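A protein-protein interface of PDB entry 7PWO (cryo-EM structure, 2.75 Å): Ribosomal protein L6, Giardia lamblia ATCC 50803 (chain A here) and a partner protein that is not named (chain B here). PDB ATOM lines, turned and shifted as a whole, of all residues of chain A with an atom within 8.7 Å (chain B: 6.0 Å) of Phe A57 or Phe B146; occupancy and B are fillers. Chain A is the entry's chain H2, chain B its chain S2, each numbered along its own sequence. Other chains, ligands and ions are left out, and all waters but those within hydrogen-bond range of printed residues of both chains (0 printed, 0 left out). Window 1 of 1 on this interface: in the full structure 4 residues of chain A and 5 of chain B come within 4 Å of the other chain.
Leu A3 touches Val B144. Leu A3 touches Phe B146 (CD1 to CD1, 3.9 Å). Trp A56 touches Pro B147 (CD2 to CD, 3.8 Å). Phe A57 touches Phe B146 (CZ to CB, 3.9 Å). Phe A57 touches Pro B147 (CZ to O, 3.4 Å). Pro B149 touches Phe A57 (CA to CE2, 3.7 Å).
O of Phe A57 sits at hydrogen-bond distance from NH2 of Arg A62 (2.5 Å). The backbone NH of Phe A57 sits at hydrogen-bond distance from the backbone carbonyl oxygen of Leu A3.
Hydrophobic or aromatic side chains of chain A that line the printed part of chain B: Leu A3, Trp A56 and Phe A57. Of the 7 printed residues of chain B, 4 touch a printed residue of chain A.
Printed residues of chain B within 4 Å of Leu A3: Val B144 (3.6 Å) and Phe B146 (3.9 Å). Ser A5 touches none of the printed residues of chain B. Printed residues of chain B within 4 Å of Trp A56: Pro B147 (3.8 Å). Phe A57 touches three residues of chain B. Phe B139 touches none of the printed residues of chain A. Of the printed residues of chain A, Val B144 touches Leu A3. Phe B146 touches just these residues of chain A: Leu A3 and Phe A57. Pro B147 touches just these residues of chain A: Trp A56 (3.8 Å) and Phe A57 (3.4 Å). Printed residues of chain A within 4 Å of Pro B149: Phe A57. The nearest residue of chain B that does not touch Phe A57 is His B148 (4.6 Å). The nearest residue of chain A that does not touch Phe B146 is Trp A56 (4.5 Å). The nearest printed residue of chain A that does not touch Val B144 is Trp A56 (8.0 Å).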
ATOM      1  N   PRO A   2      22.919  13.692  -3.114  1.00  0.00           N
ATOM      2  CA  PRO A   2      24.347  13.491  -3.345  1.00  0.00           C
ATOM      3  C   PRO A   2      25.169  14.721  -3.002  1.00  0.00           C
ATOM      4  O   PRO A   2      24.627  15.678  -2.457  1.00  0.00           O
ATOM      5  CB  PRO A   2      24.416  13.172  -4.842  1.00  0.00           C
ATOM      6  CG  PRO A   2      23.094  12.596  -5.151  1.00  0.00           C
ATOM      7  CD  PRO A   2      22.120  13.356  -4.305  1.00  0.00           C
ATOM      8  N   LEU A   3      26.469  14.675  -3.284  1.00  0.00           N
ATOM      9  CA  LEU A   3      27.335  15.832  -3.115  1.00  0.00           C
ATOM     10  C   LEU A   3      27.393  16.704  -4.355  1.00  0.00           C
ATOM     11  O   LEU A   3      27.802  17.865  -4.262  1.00  0.00           O
ATOM     12  CB  LEU A   3      28.761  15.389  -2.759  1.00  0.00           C
ATOM     13  CG  LEU A   3      28.920  14.460  -1.562  1.00  0.00           C
ATOM     14  CD1 LEU A   3      30.198  13.654  -1.612  1.00  0.00           C
ATOM     15  CD2 LEU A   3      28.842  15.267  -0.276  1.00  0.00           C
ATOM     16  N   CYS A   4      26.991  16.173  -5.501  1.00  0.00           N
ATOM     17  CA  CYS A   4      27.065  16.891  -6.757  1.00  0.00           C
ATOM     18  C   CYS A   4      25.774  16.655  -7.528  1.00  0.00           C
ATOM     19  O   CYS A   4      25.013  15.731  -7.242  1.00  0.00           O
ATOM     20  CB  CYS A   4      28.284  16.442  -7.567  1.00  0.00           C
ATOM     21  SG  CYS A   4      28.541  17.301  -9.121  1.00  0.00           S
ATOM     22  N   SER A   5      25.514  17.535  -8.483  1.00  0.00           N
ATOM     23  CA  SER A   5      24.476  17.303  -9.479  1.00  0.00           C
ATOM     24  C   SER A   5      24.969  17.882 -10.790  1.00  0.00           C
ATOM     25  O   SER A   5      25.351  19.052 -10.832  1.00  0.00           O
ATOM     26  CB  SER A   5      23.146  17.944  -9.070  1.00  0.00           C
ATOM     27  OG  SER A   5      22.083  17.442  -9.847  1.00  0.00           O
ATOM     28  N   PRO A  41      25.975  29.978  -9.110  1.00  0.00           N
ATOM     29  CA  PRO A  41      27.180  29.197  -8.802  1.00  0.00           C
ATOM     30  C   PRO A  41      27.262  27.941  -9.650  1.00  0.00           C
ATOM     31  O   PRO A  41      26.382  27.078  -9.574  1.00  0.00           O
ATOM     32  CB  PRO A  41      27.016  28.856  -7.315  1.00  0.00           C
ATOM     33  CG  PRO A  41      25.748  29.533  -6.867  1.00  0.00           C
ATOM     34  CD  PRO A  41      24.934  29.786  -8.091  1.00  0.00           C
ATOM     35  N   ALA A  54      28.014  21.414 -13.366  1.00  0.00           N
ATOM     36  CA  ALA A  54      27.872  20.741 -12.084  1.00  0.00           C
ATOM     37  C   ALA A  54      27.620  21.742 -10.965  1.00  0.00           C
ATOM     38  O   ALA A  54      28.037  22.900 -11.028  1.00  0.00           O
ATOM     39  CB  ALA A  54      29.110  19.915 -11.750  1.00  0.00           C
ATOM     40  N   VAL A  55      26.921  21.273  -9.936  1.00  0.00           N
ATOM     41  CA  VAL A  55      26.611  22.061  -8.752  1.00  0.00           C
ATOM     42  C   VAL A  55      26.932  21.212  -7.533  1.00  0.00           C
ATOM     43  O   VAL A  55      26.384  20.116  -7.377  1.00  0.00           O
ATOM     44  CB  VAL A  55      25.141  22.518  -8.723  1.00  0.00           C
ATOM     45  CG1 VAL A  55      24.850  23.240  -7.435  1.00  0.00           C
ATOM     46  CG2 VAL A  55      24.835  23.413  -9.901  1.00  0.00           C
ATOM     47  N   TRP A  56      27.818  21.711  -6.679  1.00  0.00           N
ATOM     48  CA  TRP A  56      28.195  21.029  -5.450  1.00  0.00           C
ATOM     49  C   TRP A  56      27.271  21.425  -4.312  1.00  0.00           C
ATOM     50  O   TRP A  56      26.937  22.599  -4.155  1.00  0.00           O
ATOM     51  CB  TRP A  56      29.631  21.362  -5.069  1.00  0.00           C
ATOM     52  CG  TRP A  56      30.661  20.821  -5.986  1.00  0.00           C
ATOM     53  CD1 TRP A  56      31.371  21.515  -6.913  1.00  0.00           C
ATOM     54  CD2 TRP A  56      31.151  19.476  -6.030  1.00  0.00           C
ATOM     55  NE1 TRP A  56      32.257  20.685  -7.551  1.00  0.00           N
ATOM     56  CE2 TRP A  56      32.142  19.427  -7.025  1.00  0.00           C
ATOM     57  CE3 TRP A  56      30.833  18.307  -5.339  1.00  0.00           C
ATOM     58  CZ2 TRP A  56      32.819  18.262  -7.341  1.00  0.00           C
ATOM     59  CZ3 TRP A  56      31.502  17.160  -5.651  1.00  0.00           C
ATOM     60  CH2 TRP A  56      32.488  17.140  -6.644  1.00  0.00           C
ATOM     61  N   PHE A  57      26.865  20.436  -3.520  1.00  0.00           N
ATOM     62  CA  PHE A  57      26.036  20.600  -2.330  1.00  0.00           C
ATOM     63  C   PHE A  57      24.719  21.279  -2.667  1.00  0.00           C
ATOM     64  O   PHE A  57      24.515  22.439  -2.287  1.00  0.00           O
ATOM     65  CB  PHE A  57      26.758  21.434  -1.270  1.00  0.00           C
ATOM     66  CG  PHE A  57      28.139  20.958  -0.955  1.00  0.00           C
ATOM     67  CD1 PHE A  57      28.365  19.657  -0.567  1.00  0.00           C
ATOM     68  CD2 PHE A  57      29.218  21.813  -1.083  1.00  0.00           C
ATOM     69  CE1 PHE A  57      29.639  19.227  -0.284  1.00  0.00           C
ATOM     70  CE2 PHE A  57      30.488  21.385  -0.813  1.00  0.00           C
ATOM     71  CZ  PHE A  57      30.700  20.089  -0.411  1.00  0.00           C
ATOM     72  N   PRO A  58      23.813  20.624  -3.385  1.00  0.00           N
ATOM     73  CA  PRO A  58      22.493  21.205  -3.599  1.00  0.00           C
ATOM     74  C   PRO A  58      21.629  21.043  -2.359  1.00  0.00           C
ATOM     75  O   PRO A  58      21.834  20.155  -1.532  1.00  0.00           O
ATOM     76  CB  PRO A  58      21.933  20.394  -4.775  1.00  0.00           C
ATOM     77  CG  PRO A  58      23.044  19.497  -5.218  1.00  0.00           C
ATOM     78  CD  PRO A  58      23.930  19.322  -4.055  1.00  0.00           C
ATOM     79  N   ARG A  59      20.660  21.944  -2.225  1.00  0.00           N
ATOM     80  CA  ARG A  59      19.710  21.846  -1.129  1.00  0.00           C
ATOM     81  C   ARG A  59      18.283  22.196  -1.529  1.00  0.00           C
ATOM     82  O   ARG A  59      17.380  22.089  -0.696  1.00  0.00           O
ATOM     83  CB  ARG A  59      20.166  22.741   0.030  1.00  0.00           C
ATOM     84  CG  ARG A  59      19.574  22.388   1.361  1.00  0.00           C
ATOM     85  CD  ARG A  59      20.386  22.974   2.508  1.00  0.00           C
ATOM     86  NE  ARG A  59      19.610  22.964   3.742  1.00  0.00           N
ATOM     87  CZ  ARG A  59      19.297  21.874   4.425  1.00  0.00           C
ATOM     88  NH1 ARG A  59      19.720  20.682   4.020  1.00  0.00           N
ATOM     89  NH2 ARG A  59      18.573  21.979   5.529  1.00  0.00           N
ATOM     90  N   GLY A  60      18.041  22.585  -2.763  1.00  0.00           N
ATOM     91  CA  GLY A  60      16.750  23.116  -3.123  1.00  0.00           C
ATOM     92  C   GLY A  60      16.731  23.426  -4.596  1.00  0.00           C
ATOM     93  O   GLY A  60      17.125  22.585  -5.407  1.00  0.00           O
ATOM     94  N   ARG A  62      18.673  24.851  -6.234  1.00  0.00           N
ATOM     95  CA  ARG A  62      20.000  24.748  -6.834  1.00  0.00           C
ATOM     96  C   ARG A  62      20.154  23.480  -7.655  1.00  0.00           C
ATOM     97  O   ARG A  62      21.001  23.430  -8.548  1.00  0.00           O
ATOM     98  CB  ARG A  62      21.084  24.782  -5.766  1.00  0.00           C
ATOM     99  CG  ARG A  62      21.028  25.966  -4.864  1.00  0.00           C
ATOM    100  CD  ARG A  62      22.422  26.432  -4.519  1.00  0.00           C
ATOM    101  NE  ARG A  62      23.032  25.613  -3.484  1.00  0.00           N
ATOM    102  CZ  ARG A  62      24.309  25.697  -3.128  1.00  0.00           C
ATOM    103  NH1 ARG A  62      25.105  26.571  -3.717  1.00  0.00           N
ATOM    104  NH2 ARG A  62      24.788  24.913  -2.174  1.00  0.00           N
ATOM    105  N   ASN A  63      19.350  22.462  -7.365  1.00  0.00           N
ATOM    106  CA  ASN A  63      19.285  21.251  -8.166  1.00  0.00           C
ATOM    107  C   ASN A  63      18.620  21.482  -9.519  1.00  0.00           C
ATOM    108  O   ASN A  63      18.675  20.595 -10.377  1.00  0.00           O
ATOM    109  CB  ASN A  63      18.541  20.180  -7.368  1.00  0.00           C
ATOM    110  CG  ASN A  63      18.754  18.784  -7.907  1.00  0.00           C
ATOM    111  OD1 ASN A  63      17.869  18.216  -8.537  1.00  0.00           O
ATOM    112  ND2 ASN A  63      19.915  18.211  -7.633  1.00  0.00           N
ATOM    113  N   PHE B 139      28.566   8.428   2.284  1.00  0.00           N
ATOM    114  CA  PHE B 139      29.913   8.403   2.822  1.00  0.00           C
ATOM    115  C   PHE B 139      30.417   6.995   3.095  1.00  0.00           C
ATOM    116  O   PHE B 139      31.574   6.832   3.494  1.00  0.00           O
ATOM    117  CB  PHE B 139      29.955   9.240   4.101  1.00  0.00           C
ATOM    118  CG  PHE B 139      29.730  10.694   3.869  1.00  0.00           C
ATOM    119  CD1 PHE B 139      30.768  11.504   3.457  1.00  0.00           C
ATOM    120  CD2 PHE B 139      28.471  11.249   4.018  1.00  0.00           C
ATOM    121  CE1 PHE B 139      30.565  12.835   3.226  1.00  0.00           C
ATOM    122  CE2 PHE B 139      28.268  12.584   3.786  1.00  0.00           C
ATOM    123  CZ  PHE B 139      29.316  13.375   3.389  1.00  0.00           C
ATOM    124  N   VAL B 144      35.433   8.966  -1.754  1.00  0.00           N
ATOM    125  CA  VAL B 144      34.525  10.106  -1.680  1.00  0.00           C
ATOM    126  C   VAL B 144      35.340  11.391  -1.578  1.00  0.00           C
ATOM    127  O   VAL B 144      36.249  11.504  -0.749  1.00  0.00           O
ATOM    128  CB  VAL B 144      33.534   9.947  -0.513  1.00  0.00           C
ATOM    129  CG1 VAL B 144      34.232   9.965   0.836  1.00  0.00           C
ATOM    130  CG2 VAL B 144      32.464  11.023  -0.578  1.00  0.00           C
ATOM    131  N   ARG B 145      35.042  12.350  -2.457  1.00  0.00           N
ATOM    132  CA  ARG B 145      35.734  13.632  -2.515  1.00  0.00           C
ATOM    133  C   ARG B 145      34.732  14.762  -2.635  1.00  0.00           C
ATOM    134  O   ARG B 145      33.742  14.658  -3.364  1.00  0.00           O
ATOM    135  CB  ARG B 145      36.684  13.733  -3.706  1.00  0.00           C
ATOM    136  CG  ARG B 145      37.367  12.458  -4.111  1.00  0.00           C
ATOM    137  CD  ARG B 145      38.211  12.678  -5.349  1.00  0.00           C
ATOM    138  NE  ARG B 145      39.428  13.436  -5.081  1.00  0.00           N
ATOM    139  CZ  ARG B 145      39.812  14.502  -5.775  1.00  0.00           C
ATOM    140  NH1 ARG B 145      39.089  14.932  -6.797  1.00  0.00           N
ATOM    141  NH2 ARG B 145      40.934  15.126  -5.456  1.00  0.00           N
ATOM    142  N   PHE B 146      35.012  15.858  -1.942  1.00  0.00           N
ATOM    143  CA  PHE B 146      34.271  17.086  -2.141  1.00  0.00           C
ATOM    144  C   PHE B 146      35.162  18.269  -1.804  1.00  0.00           C
ATOM    145  O   PHE B 146      36.059  18.150  -0.962  1.00  0.00           O
ATOM    146  CB  PHE B 146      32.967  17.110  -1.324  1.00  0.00           C
ATOM    147  CG  PHE B 146      33.109  16.644   0.106  1.00  0.00           C
ATOM    148  CD1 PHE B 146      33.068  15.289   0.411  1.00  0.00           C
ATOM    149  CD2 PHE B 146      33.231  17.550   1.142  1.00  0.00           C
ATOM    150  CE1 PHE B 146      33.179  14.850   1.715  1.00  0.00           C
ATOM    151  CE2 PHE B 146      33.344  17.113   2.454  1.00  0.00           C
ATOM    152  CZ  PHE B 146      33.316  15.768   2.739  1.00  0.00           C
ATOM    153  N   PRO B 147      34.982  19.396  -2.481  1.00  0.00           N
ATOM    154  CA  PRO B 147      35.693  20.611  -2.087  1.00  0.00           C
ATOM    155  C   PRO B 147      35.126  21.153  -0.791  1.00  0.00           C
ATOM    156  O   PRO B 147      33.970  20.896  -0.448  1.00  0.00           O
ATOM    157  CB  PRO B 147      35.436  21.565  -3.256  1.00  0.00           C
ATOM    158  CG  PRO B 147      34.162  21.102  -3.844  1.00  0.00           C
ATOM    159  CD  PRO B 147      34.074  19.621  -3.617  1.00  0.00           C
ATOM    160  N   HIS B 148      35.946  21.925  -0.078  1.00  0.00           N
ATOM    161  CA  HIS B 148      35.600  22.352   1.267  1.00  0.00           C
ATOM    162  C   HIS B 148      34.246  23.059   1.270  1.00  0.00           C
ATOM    163  O   HIS B 148      34.031  23.983   0.477  1.00  0.00           O
ATOM    164  CB  HIS B 148      36.677  23.275   1.832  1.00  0.00           C
ATOM    165  CG  HIS B 148      36.697  23.342   3.328  1.00  0.00           C
ATOM    166  ND1 HIS B 148      35.596  23.706   4.070  1.00  0.00           N
ATOM    167  CD2 HIS B 148      37.684  23.096   4.219  1.00  0.00           C
ATOM    168  CE1 HIS B 148      35.903  23.684   5.353  1.00  0.00           C
ATOM    169  NE2 HIS B 148      37.163  23.314   5.471  1.00  0.00           N
ATOM    170  N   PRO B 149      33.307  22.641   2.124  1.00  0.00           N
ATOM    171  CA  PRO B 149      31.946  23.190   2.060  1.00  0.00           C
ATOM    172  C   PRO B 149      31.769  24.560   2.693  1.00  0.00           C
ATOM    173  O   PRO B 149      30.677  25.123   2.572  1.00  0.00           O
ATOM    174  CB  PRO B 149      31.113  22.135   2.803  1.00  0.00           C
ATOM    175  CG  PRO B 149      32.078  21.407   3.660  1.00  0.00           C
ATOM    176  CD  PRO B 149      33.390  21.438   2.967  1.00  0.00           C
